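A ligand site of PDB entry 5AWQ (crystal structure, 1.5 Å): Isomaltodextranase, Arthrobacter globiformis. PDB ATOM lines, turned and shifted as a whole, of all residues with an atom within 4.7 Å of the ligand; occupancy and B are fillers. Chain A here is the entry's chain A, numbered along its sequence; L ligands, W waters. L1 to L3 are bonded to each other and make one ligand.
OD2 of Asp 201 sits close to O4 of LG2 L2. CE1 of Tyr 44 touches O3 of LG2 L2 (3.2 Å). CA of Gly 82 touches O4 of LG3 L3 (3.5 Å). OH of Tyr 124 touches C6 of LG2 L2, at 3.8 Å. Phe 160 touches the ligand. Phe 202 touches the ligand. OD1 of Asn 213 touches O2 of LIG L1, 3.6 Å away. CE of SME 247 touches O3 of LIG L1, at 3.5 Å. Hydrophobic or aromatic side chains that line the ligand: Tyr 44, Trp 83, Ile 84, Phe 160, Phe 202 and Trp 289. Within 4 Å of the ligand: Tyr 44, Asp 81, Gly 82, Trp 83, Ile 84, Glu 85, Tyr 124, Phe 160, Asp 201, Phe 202, Asp 211, Asn 213, SME 247, Arg 265, Asp 269 and Trp 289. The nearest printed residue that does not touch the ligand is Trp 205 (4.02 Å).
OD1 of Asp 269 is in salt-bridge range of NH2 of Arg 265 (2.8 Å). OD1 of Asp 211 is in hydrogen-bond range of N of Asn 213, at 2.8 Å. OD2 of Asp 211 is in hydrogen-bond range of NE1 of Trp 205, 2.9 Å away. NE1 of Trp 83 is in hydrogen-bond range of OD1 of Asn 51 (2.9 Å). The guanidinium group (NH1) of Arg 265 lies within salt-bridge range of the side-chain carboxylate (OD1) of Asp 316, at 3.1 Å. The side-chain carboxylate (OD2) of Asp 201 lies within hydrogen-bond range of the side-chain hydroxyl (OH) of Tyr 124. OE of SME 247 lies within hydrogen-bond range of the backbone NH (N) of Trp 205, at 2.9 Å.
Water W10 lies within hydrogen-bond range of an oxygen (O1) of LG2 L2 (2.5 Å), the side-chain carboxylate (OD1) of Asp 201 (2.7 Å) and the backbone carbonyl oxygen (O) of Val 246 (2.8 Å). Water W3 bridges an oxygen (O2) of LG2 L2 (2.6 Å) and the side-chain carboxylate of Asp 316 (2.7 Å). Water W9 bridges an oxygen (O1) of LG3 L3 (2.7 Å) and the side-chain amide oxygen of Asn 51 (2.8 Å). Water W11 bridges O2 of LIG L1 (2.8 Å) and OD1 of Asn 213 (2.9 Å). Water W4 lies within hydrogen-bond range of an oxygen (O1) of LIG L1 and the side-chain carboxylate of Asp 269. Water W7 lies within hydrogen-bond range of the side-chain carboxylate (OD1) of Asp 81 (2.7 Å) and an oxygen (O2) of LG2 L2 (2.9 Å).
OD1 of Asp 269 is in hydrogen-bond range of O1 of LG2 L2 (2.5 Å). OE2 of Glu 85 sits at hydrogen-bond distance from O5 of LG3 L3 (2.6 Å). The side-chain carboxylate of Asp 211 is in hydrogen-bond range of an oxygen (O2) of LIG L1 (2.7 Å). The side-chain carboxylate of Asp 81 lies within hydrogen-bond range of an oxygen (O3) of LG2 L2 (2.8 Å). The backbone NH (N) of Trp 83 is in hydrogen-bond range of an oxygen (O4) of LG3 L3, 2.9 Å away. An oxygen (O5) of LG3 L3 lies within hydrogen-bond range of the backbone NH of Ile 84 (2.9 Å). NH1 of Arg 265 is in hydrogen-bond range of O2 of LG2 L2. The indole nitrogen of Trp 289 is in hydrogen-bond range of an oxygen (O3) of LIG L1 (3.2 Å).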
ATOM      1  N   TYR A  44      10.475 -14.463  11.405  1.00  0.00           N
ATOM      2  CA  TYR A  44      11.918 -14.470  11.145  1.00  0.00           C
ATOM      3  C   TYR A  44      12.420 -13.181  10.510  1.00  0.00           C
ATOM      4  O   TYR A  44      13.545 -12.783  10.781  1.00  0.00           O
ATOM      5  CB  TYR A  44      12.238 -15.641  10.240  1.00  0.00           C
ATOM      6  CG  TYR A  44      13.681 -15.969   9.990  1.00  0.00           C
ATOM      7  CD1 TYR A  44      14.388 -16.785  10.851  1.00  0.00           C
ATOM      8  CD2 TYR A  44      14.352 -15.485   8.851  1.00  0.00           C
ATOM      9  CE1 TYR A  44      15.703 -17.130  10.602  1.00  0.00           C
ATOM     10  CE2 TYR A  44      15.660 -15.827   8.590  1.00  0.00           C
ATOM     11  CZ  TYR A  44      16.339 -16.653   9.466  1.00  0.00           C
ATOM     12  OH  TYR A  44      17.641 -17.014   9.214  1.00  0.00           O
ATOM     13  N   ASN A  51      18.277 -10.063  15.626  1.00  0.00           N
ATOM     14  CA  ASN A  51      18.830 -11.060  16.539  1.00  0.00           C
ATOM     15  C   ASN A  51      18.165 -10.965  17.905  1.00  0.00           C
ATOM     16  O   ASN A  51      18.827 -10.897  18.936  1.00  0.00           O
ATOM     17  CB  ASN A  51      20.347 -10.930  16.643  1.00  0.00           C
ATOM     18  CG  ASN A  51      20.988 -12.095  17.397  1.00  0.00           C
ATOM     19  OD1 ASN A  51      20.425 -13.189  17.457  1.00  0.00           O
ATOM     20  ND2 ASN A  51      22.138 -11.847  17.995  1.00  0.00           N
ATOM     21  N   ASP A  81       8.955 -18.142  15.797  1.00  0.00           N
ATOM     22  CA  ASP A  81      10.205 -18.803  15.481  1.00  0.00           C
ATOM     23  C   ASP A  81      11.051 -18.846  16.763  1.00  0.00           C
ATOM     24  O   ASP A  81      10.485 -18.964  17.870  1.00  0.00           O
ATOM     25  CB  ASP A  81      10.902 -18.113  14.283  1.00  0.00           C
ATOM     26  CG  ASP A  81      11.973 -18.974  13.656  1.00  0.00           C
ATOM     27  OD1 ASP A  81      11.625 -19.892  12.878  1.00  0.00           O
ATOM     28  OD2 ASP A  81      13.157 -18.734  13.951  1.00  0.00           O
ATOM     29  N   GLY A  82      12.370 -18.797  16.635  1.00  0.00           N
ATOM     30  CA  GLY A  82      13.269 -18.921  17.766  1.00  0.00           C
ATOM     31  C   GLY A  82      13.387 -17.706  18.649  1.00  0.00           C
ATOM     32  O   GLY A  82      12.429 -16.948  18.826  1.00  0.00           O
ATOM     33  N   TRP A  83      14.572 -17.561  19.238  1.00  0.00           N
ATOM     34  CA  TRP A  83      14.829 -16.544  20.247  1.00  0.00           C
ATOM     35  C   TRP A  83      13.846 -16.759  21.410  1.00  0.00           C
ATOM     36  O   TRP A  83      13.252 -15.822  21.912  1.00  0.00           O
ATOM     37  CB  TRP A  83      14.759 -15.114  19.655  1.00  0.00           C
ATOM     38  CG  TRP A  83      15.831 -14.890  18.650  1.00  0.00           C
ATOM     39  CD1 TRP A  83      17.068 -14.349  18.888  1.00  0.00           C
ATOM     40  CD2 TRP A  83      15.816 -15.253  17.258  1.00  0.00           C
ATOM     41  NE1 TRP A  83      17.803 -14.328  17.731  1.00  0.00           N
ATOM     42  CE2 TRP A  83      17.058 -14.883  16.719  1.00  0.00           C
ATOM     43  CE3 TRP A  83      14.864 -15.842  16.421  1.00  0.00           C
ATOM     44  CZ2 TRP A  83      17.385 -15.124  15.384  1.00  0.00           C
ATOM     45  CZ3 TRP A  83      15.191 -16.075  15.104  1.00  0.00           C
ATOM     46  CH2 TRP A  83      16.427 -15.700  14.595  1.00  0.00           C
ATOM     47  N   ILE A  84      13.712 -18.023  21.826  1.00  0.00           N
ATOM     48  CA  ILE A  84      12.791 -18.421  22.903  1.00  0.00           C
ATOM     49  C   ILE A  84      13.457 -18.663  24.267  1.00  0.00           C
ATOM     50  O   ILE A  84      12.787 -19.066  25.219  1.00  0.00           O
ATOM     51  CB  ILE A  84      11.875 -19.614  22.504  1.00  0.00           C
ATOM     52  CG1 ILE A  84      12.657 -20.815  21.904  1.00  0.00           C
ATOM     53  CG2 ILE A  84      10.790 -19.164  21.542  1.00  0.00           C
ATOM     54  CD1 ILE A  84      13.691 -21.440  22.802  1.00  0.00           C
ATOM     55  N   GLU A  85      14.734 -18.354  24.399  1.00  0.00           N
ATOM     56  CA  GLU A  85      15.390 -18.524  25.698  1.00  0.00           C
ATOM     57  C   GLU A  85      14.722 -17.664  26.784  1.00  0.00           C
ATOM     58  O   GLU A  85      14.653 -18.065  27.934  1.00  0.00           O
ATOM     59  CB  GLU A  85      16.880 -18.177  25.610  1.00  0.00           C
ATOM     60  CG  GLU A  85      17.762 -19.285  25.042  1.00  0.00           C
ATOM     61  CD  GLU A  85      17.750 -19.421  23.518  1.00  0.00           C
ATOM     62  OE1 GLU A  85      18.472 -20.316  23.037  1.00  0.00           O
ATOM     63  OE2 GLU A  85      17.034 -18.669  22.828  1.00  0.00           O
ATOM     64  N   TYR A 124       6.664 -22.324  17.047  1.00  0.00           N
ATOM     65  CA  TYR A 124       8.002 -22.918  17.037  1.00  0.00           C
ATOM     66  C   TYR A 124       8.337 -23.309  18.476  1.00  0.00           C
ATOM     67  O   TYR A 124       8.491 -22.445  19.349  1.00  0.00           O
ATOM     68  CB  TYR A 124       8.995 -21.885  16.488  1.00  0.00           C
ATOM     69  CG  TYR A 124      10.476 -22.199  16.548  1.00  0.00           C
ATOM     70  CD1 TYR A 124      11.206 -22.086  17.732  1.00  0.00           C
ATOM     71  CD2 TYR A 124      11.183 -22.511  15.374  1.00  0.00           C
ATOM     72  CE1 TYR A 124      12.573 -22.310  17.756  1.00  0.00           C
ATOM     73  CE2 TYR A 124      12.549 -22.730  15.406  1.00  0.00           C
ATOM     74  CZ  TYR A 124      13.237 -22.617  16.592  1.00  0.00           C
ATOM     75  OH  TYR A 124      14.604 -22.816  16.638  1.00  0.00           O
ATOM     76  N   TRP A 129      12.760 -29.510  25.050  1.00  0.00           N
ATOM     77  CA  TRP A 129      13.349 -28.435  25.828  1.00  0.00           C
ATOM     78  C   TRP A 129      12.648 -28.372  27.176  1.00  0.00           C
ATOM     79  O   TRP A 129      11.405 -28.455  27.240  1.00  0.00           O
ATOM     80  CB  TRP A 129      13.262 -27.067  25.164  1.00  0.00           C
ATOM     81  CG  TRP A 129      14.268 -26.809  24.081  1.00  0.00           C
ATOM     82  CD1 TRP A 129      15.555 -27.242  24.035  1.00  0.00           C
ATOM     83  CD2 TRP A 129      14.061 -26.014  22.908  1.00  0.00           C
ATOM     84  NE1 TRP A 129      16.169 -26.763  22.888  1.00  0.00           N
ATOM     85  CE2 TRP A 129      15.284 -25.998  22.197  1.00  0.00           C
ATOM     86  CE3 TRP A 129      12.983 -25.279  22.400  1.00  0.00           C
ATOM     87  CZ2 TRP A 129      15.429 -25.317  20.998  1.00  0.00           C
ATOM     88  CZ3 TRP A 129      13.142 -24.606  21.182  1.00  0.00           C
ATOM     89  CH2 TRP A 129      14.359 -24.632  20.501  1.00  0.00           C
ATOM     90  N   PHE A 160      20.937 -27.293  26.482  1.00  0.00           N
ATOM     91  CA  PHE A 160      20.935 -26.986  25.069  1.00  0.00           C
ATOM     92  C   PHE A 160      22.022 -25.952  24.801  1.00  0.00           C
ATOM     93  O   PHE A 160      22.092 -24.932  25.487  1.00  0.00           O
ATOM     94  CB  PHE A 160      19.557 -26.437  24.695  1.00  0.00           C
ATOM     95  CG  PHE A 160      19.494 -25.746  23.367  1.00  0.00           C
ATOM     96  CD1 PHE A 160      19.748 -26.433  22.197  1.00  0.00           C
ATOM     97  CD2 PHE A 160      19.143 -24.399  23.300  1.00  0.00           C
ATOM     98  CE1 PHE A 160      19.674 -25.788  20.977  1.00  0.00           C
ATOM     99  CE2 PHE A 160      19.083 -23.753  22.079  1.00  0.00           C
ATOM    100  CZ  PHE A 160      19.331 -24.456  20.927  1.00  0.00           C
ATOM    101  N   ASP A 201      12.600 -27.586  16.148  1.00  0.00           N
ATOM    102  CA  ASP A 201      13.958 -27.313  15.703  1.00  0.00           C
ATOM    103  C   ASP A 201      14.980 -27.889  16.678  1.00  0.00           C
ATOM    104  O   ASP A 201      14.654 -28.293  17.794  1.00  0.00           O
ATOM    105  CB  ASP A 201      14.158 -25.793  15.587  1.00  0.00           C
ATOM    106  CG  ASP A 201      15.296 -25.382  14.672  1.00  0.00           C
ATOM    107  OD1 ASP A 201      15.921 -26.249  14.029  1.00  0.00           O
ATOM    108  OD2 ASP A 201      15.511 -24.161  14.578  1.00  0.00           O
ATOM    109  N   PHE A 202      16.217 -27.967  16.194  1.00  0.00           N
ATOM    110  CA  PHE A 202      17.381 -28.302  16.993  1.00  0.00           C
ATOM    111  C   PHE A 202      17.460 -29.778  17.409  1.00  0.00           C
ATOM    112  O   PHE A 202      18.285 -30.126  18.225  1.00  0.00           O
ATOM    113  CB  PHE A 202      17.538 -27.364  18.194  1.00  0.00           C
ATOM    114  CG  PHE A 202      18.012 -25.986  17.815  1.00  0.00           C
ATOM    115  CD1 PHE A 202      19.346 -25.781  17.499  1.00  0.00           C
ATOM    116  CD2 PHE A 202      17.139 -24.938  17.753  1.00  0.00           C
ATOM    117  CE1 PHE A 202      19.809 -24.537  17.168  1.00  0.00           C
ATOM    118  CE2 PHE A 202      17.586 -23.680  17.384  1.00  0.00           C
ATOM    119  CZ  PHE A 202      18.913 -23.490  17.085  1.00  0.00           C
ATOM    120  N   TRP A 205      21.091 -31.123  16.949  1.00  0.00           N
ATOM    121  CA  TRP A 205      21.912 -30.759  18.119  1.00  0.00           C
ATOM    122  C   TRP A 205      21.611 -31.662  19.311  1.00  0.00           C
ATOM    123  O   TRP A 205      22.524 -32.086  20.004  1.00  0.00           O
ATOM    124  CB  TRP A 205      21.718 -29.297  18.521  1.00  0.00           C
ATOM    125  CG  TRP A 205      22.309 -28.302  17.564  1.00  0.00           C
ATOM    126  CD1 TRP A 205      22.594 -28.488  16.249  1.00  0.00           C
ATOM    127  CD2 TRP A 205      22.678 -26.948  17.876  1.00  0.00           C
ATOM    128  NE1 TRP A 205      23.092 -27.336  15.707  1.00  0.00           N
ATOM    129  CE2 TRP A 205      23.163 -26.373  16.669  1.00  0.00           C
ATOM    130  CE3 TRP A 205      22.663 -26.171  19.032  1.00  0.00           C
ATOM    131  CZ2 TRP A 205      23.626 -25.053  16.600  1.00  0.00           C
ATOM    132  CZ3 TRP A 205      23.112 -24.851  18.963  1.00  0.00           C
ATOM    133  CH2 TRP A 205      23.590 -24.312  17.762  1.00  0.00           C
ATOM    134  N   ASP A 211      27.390 -29.424  15.290  1.00  0.00           N
ATOM    135  CA  ASP A 211      26.948 -28.732  14.082  1.00  0.00           C
ATOM    136  C   ASP A 211      28.165 -28.523  13.178  1.00  0.00           C
ATOM    137  O   ASP A 211      29.211 -28.045  13.635  1.00  0.00           O
ATOM    138  CB  ASP A 211      26.299 -27.396  14.422  1.00  0.00           C
ATOM    139  CG  ASP A 211      25.603 -26.764  13.227  1.00  0.00           C
ATOM    140  OD1 ASP A 211      26.279 -26.421  12.225  1.00  0.00           O
ATOM    141  OD2 ASP A 211      24.380 -26.572  13.267  1.00  0.00           O
ATOM    142  N   ASN A 213      28.775 -26.345  11.045  1.00  0.00           N
ATOM    143  CA  ASN A 213      29.182 -24.923  10.999  1.00  0.00           C
ATOM    144  C   ASN A 213      29.948 -24.442  12.228  1.00  0.00           C
ATOM    145  O   ASN A 213      30.518 -23.360  12.194  1.00  0.00           O
ATOM    146  CB  ASN A 213      27.961 -23.987  10.920  1.00  0.00           C
ATOM    147  CG  ASN A 213      27.269 -23.981   9.584  1.00  0.00           C
ATOM    148  OD1 ASN A 213      26.070 -23.683   9.512  1.00  0.00           O
ATOM    149  ND2 ASN A 213      28.000 -24.281   8.524  1.00  0.00           N
ATOM    150  N   ILE A 214      29.898 -25.197  13.326  1.00  0.00           N
ATOM    151  CA  ILE A 214      30.355 -24.693  14.620  1.00  0.00           C
ATOM    152  C   ILE A 214      31.430 -25.582  15.250  1.00  0.00           C
ATOM    153  O   ILE A 214      32.510 -25.099  15.628  1.00  0.00           O
ATOM    154  CB  ILE A 214      29.184 -24.550  15.620  1.00  0.00           C
ATOM    155  CG1 ILE A 214      28.168 -23.536  15.097  1.00  0.00           C
ATOM    156  CG2 ILE A 214      29.728 -24.133  16.993  1.00  0.00           C
ATOM    157  CD1 ILE A 214      26.899 -23.390  15.913  1.00  0.00           C
ATOM    158  N   VAL A 246      12.671 -29.171  11.772  1.00  0.00           N
ATOM    159  CA  VAL A 246      13.389 -28.017  11.244  1.00  0.00           C
ATOM    160  C   VAL A 246      14.886 -28.274  11.136  1.00  0.00           C
ATOM    161  O   VAL A 246      15.559 -27.634  10.300  1.00  0.00           O
ATOM    162  CB  VAL A 246      13.059 -26.747  12.074  1.00  0.00           C
ATOM    163  CG1 VAL A 246      13.711 -25.496  11.472  1.00  0.00           C
ATOM    164  CG2 VAL A 246      11.549 -26.564  12.192  1.00  0.00           C
ATOM    165  N   SME A 247      15.400 -29.206  11.934  1.00  0.00           N
ATOM    166  CA  SME A 247      16.841 -29.561  11.849  1.00  0.00           C
ATOM    167  CB  SME A 247      17.613 -29.009  13.047  1.00  0.00           C
ATOM    168  CG  SME A 247      19.110 -28.971  12.712  1.00  0.00           C
ATOM    169  S   SME A 247      20.147 -28.578  14.015  1.00  0.00           S
ATOM    170  OE  SME A 247      19.604 -29.343  15.176  1.00  0.00           O
ATOM    171  CE  SME A 247      19.819 -26.909  14.221  1.00  0.00           C
ATOM    172  C   SME A 247      16.997 -31.052  11.788  1.00  0.00           C
ATOM    173  O   SME A 247      17.452 -31.705  12.749  1.00  0.00           O
ATOM    174  N   ARG A 265      13.004 -29.638   6.767  1.00  0.00           N
ATOM    175  CA  ARG A 265      13.860 -28.618   6.140  1.00  0.00           C
ATOM    176  C   ARG A 265      14.909 -29.281   5.263  1.00  0.00           C
ATOM    177  O   ARG A 265      15.553 -30.249   5.690  1.00  0.00           O
ATOM    178  CB  ARG A 265      14.529 -27.746   7.190  1.00  0.00           C
ATOM    179  CG  ARG A 265      13.699 -26.541   7.626  1.00  0.00           C
ATOM    180  CD  ARG A 265      13.852 -25.346   6.682  1.00  0.00           C
ATOM    181  NE  ARG A 265      15.251 -24.948   6.661  1.00  0.00           N
ATOM    182  CZ  ARG A 265      15.889 -24.296   7.634  1.00  0.00           C
ATOM    183  NH1 ARG A 265      15.242 -23.839   8.699  1.00  0.00           N
ATOM    184  NH2 ARG A 265      17.208 -24.116   7.525  1.00  0.00           N
ATOM    185  N   ASP A 269      19.543 -22.088   6.488  1.00  0.00           N
ATOM    186  CA  ASP A 269      18.583 -21.045   6.802  1.00  0.00           C
ATOM    187  C   ASP A 269      18.505 -19.975   5.723  1.00  0.00           C
ATOM    188  O   ASP A 269      19.518 -19.634   5.095  1.00  0.00           O
ATOM    189  CB  ASP A 269      18.989 -20.325   8.080  1.00  0.00           C
ATOM    190  CG  ASP A 269      19.021 -21.213   9.277  1.00  0.00           C
ATOM    191  OD1 ASP A 269      18.442 -22.339   9.264  1.00  0.00           O
ATOM    192  OD2 ASP A 269      19.596 -20.760  10.273  1.00  0.00           O
ATOM    193  N   TRP A 289      23.672 -32.127   8.932  1.00  0.00           N
ATOM    194  CA  TRP A 289      22.697 -31.038   8.789  1.00  0.00           C
ATOM    195  C   TRP A 289      23.382 -29.749   8.344  1.00  0.00           C
ATOM    196  O   TRP A 289      24.369 -29.344   8.934  1.00  0.00           O
ATOM    197  CB  TRP A 289      21.960 -30.746  10.115  1.00  0.00           C
ATOM    198  CG  TRP A 289      21.392 -29.344  10.129  1.00  0.00           C
ATOM    199  CD1 TRP A 289      21.926 -28.257  10.739  1.00  0.00           C
ATOM    200  CD2 TRP A 289      20.258 -28.887   9.395  1.00  0.00           C
ATOM    201  NE1 TRP A 289      21.174 -27.148  10.461  1.00  0.00           N
ATOM    202  CE2 TRP A 289      20.150 -27.507   9.623  1.00  0.00           C
ATOM    203  CE3 TRP A 289      19.300 -29.514   8.596  1.00  0.00           C
ATOM    204  CZ2 TRP A 289      19.114 -26.734   9.097  1.00  0.00           C
ATOM    205  CZ3 TRP A 289      18.285 -28.747   8.039  1.00  0.00           C
ATOM    206  CH2 TRP A 289      18.206 -27.371   8.290  1.00  0.00           C
ATOM    207  N   ASP A 316      12.174 -23.417   3.778  1.00  0.00           N
ATOM    208  CA  ASP A 316      12.358 -22.321   4.723  1.00  0.00           C
ATOM    209  C   ASP A 316      11.552 -21.087   4.359  1.00  0.00           C
ATOM    210  O   ASP A 316      10.420 -21.202   3.887  1.00  0.00           O
ATOM    211  CB  ASP A 316      13.851 -22.037   5.001  1.00  0.00           C
ATOM    212  CG  ASP A 316      14.092 -21.482   6.400  1.00  0.00           C
ATOM    213  OD1 ASP A 316      13.344 -21.824   7.337  1.00  0.00           O
ATOM    214  OD2 ASP A 316      15.052 -20.738   6.568  1.00  0.00           O
HETATM  215  C1  LIG L   1      23.562 -22.586  13.280  1.00  0.00           C
HETATM  216  C2  LIG L   1      22.728 -23.798  12.800  1.00  0.00           C
HETATM  217  C3  LIG L   1      21.389 -23.297  12.315  1.00  0.00           C
HETATM  218  C4  LIG L   1      20.666 -22.519  13.427  1.00  0.00           C
HETATM  219  C5  LIG L   1      21.557 -21.372  13.934  1.00  0.00           C
HETATM  220  C6  LIG L   1      20.987 -20.733  15.201  1.00  0.00           C
HETATM  221  O1  LIG L   1      23.904 -21.678  12.259  1.00  0.00           O
HETATM  222  O2  LIG L   1      23.369 -24.540  11.773  1.00  0.00           O
HETATM  223  O3  LIG L   1      20.598 -24.382  11.876  1.00  0.00           O
HETATM  224  O4  LIG L   1      19.433 -22.008  12.945  1.00  0.00           O
HETATM  225  O5  LIG L   1      22.842 -21.871  14.267  1.00  0.00           O
HETATM  226  O6  LIG L   1      21.574 -19.469  15.458  1.00  0.00           O
HETATM  227  C1  LG2 L   2      18.256 -22.628  13.526  1.00  0.00           C
HETATM  228  C2  LG2 L   2      17.253 -22.877  12.410  1.00  0.00           C
HETATM  229  C3  LG2 L   2      16.585 -21.589  11.920  1.00  0.00           C
HETATM  230  C4  LG2 L   2      15.999 -20.828  13.111  1.00  0.00           C
HETATM  231  C5  LG2 L   2      17.126 -20.605  14.126  1.00  0.00           C
HETATM  232  C6  LG2 L   2      16.669 -19.876  15.383  1.00  0.00           C
HETATM  233  O1  LG2 L   2      17.921 -23.528  11.342  1.00  0.00           O
HETATM  234  O2  LG2 L   2      15.600 -21.872  10.938  1.00  0.00           O
HETATM  235  O3  LG2 L   2      15.474 -19.575  12.676  1.00  0.00           O
HETATM  236  O4  LG2 L   2      17.686 -21.843  14.543  1.00  0.00           O
HETATM  237  O5  LG2 L   2      17.818 -19.515  16.150  1.00  0.00           O
HETATM  238  C1  LG3 L   3      17.501 -18.559  17.161  1.00  0.00           C
HETATM  239  C2  LG3 L   3      18.799 -17.988  17.733  1.00  0.00           C
HETATM  240  C3  LG3 L   3      19.549 -19.005  18.594  1.00  0.00           C
HETATM  241  C4  LG3 L   3      18.599 -19.552  19.650  1.00  0.00           C
HETATM  242  C5  LG3 L   3      17.389 -20.147  18.932  1.00  0.00           C
HETATM  243  C6  LG3 L   3      16.337 -20.726  19.884  1.00  0.00           C
HETATM  244  O1  LG3 L   3      19.621 -17.529  16.655  1.00  0.00           O
HETATM  245  O2  LG3 L   3      20.677 -18.387  19.206  1.00  0.00           O
HETATM  246  O3  LG3 L   3      19.212 -20.527  20.452  1.00  0.00           O
HETATM  247  O4  LG3 L   3      16.720 -19.132  18.190  1.00  0.00           O
HETATM  248  O5  LG3 L   3      15.811 -19.744  20.769  1.00  0.00           O
HETATM  249  O   HOH W   1      26.217 -20.549  13.223  1.00  0.00           O
HETATM  250  O   HOH W   2      20.415 -15.878  20.659  1.00  0.00           O
HETATM  251  O   HOH W   3      15.682 -20.073   9.119  1.00  0.00           O
HETATM  252  O   HOH W   4      22.821 -20.643   9.795  1.00  0.00           O
HETATM  253  O   HOH W   5      24.547 -20.912  16.591  1.00  0.00           O
HETATM  254  O   HOH W   6      22.995 -19.986  18.580  1.00  0.00           O
HETATM  255  O   HOH W   7      12.840 -22.047  11.831  1.00  0.00           O
HETATM  256  O   HOH W   8      21.685 -21.827  20.291  1.00  0.00           O
HETATM  257  O   HOH W   9      21.498 -15.696  17.039  1.00  0.00           O
HETATM  258  O   HOH W  10      17.355 -25.983  11.716  1.00  0.00           O
HETATM  259  O   HOH W  11      23.430 -24.722   8.978  1.00  0.00           O
HETATM  260  O   HOH W  12      19.465 -17.499  13.718  1.00  0.00           O
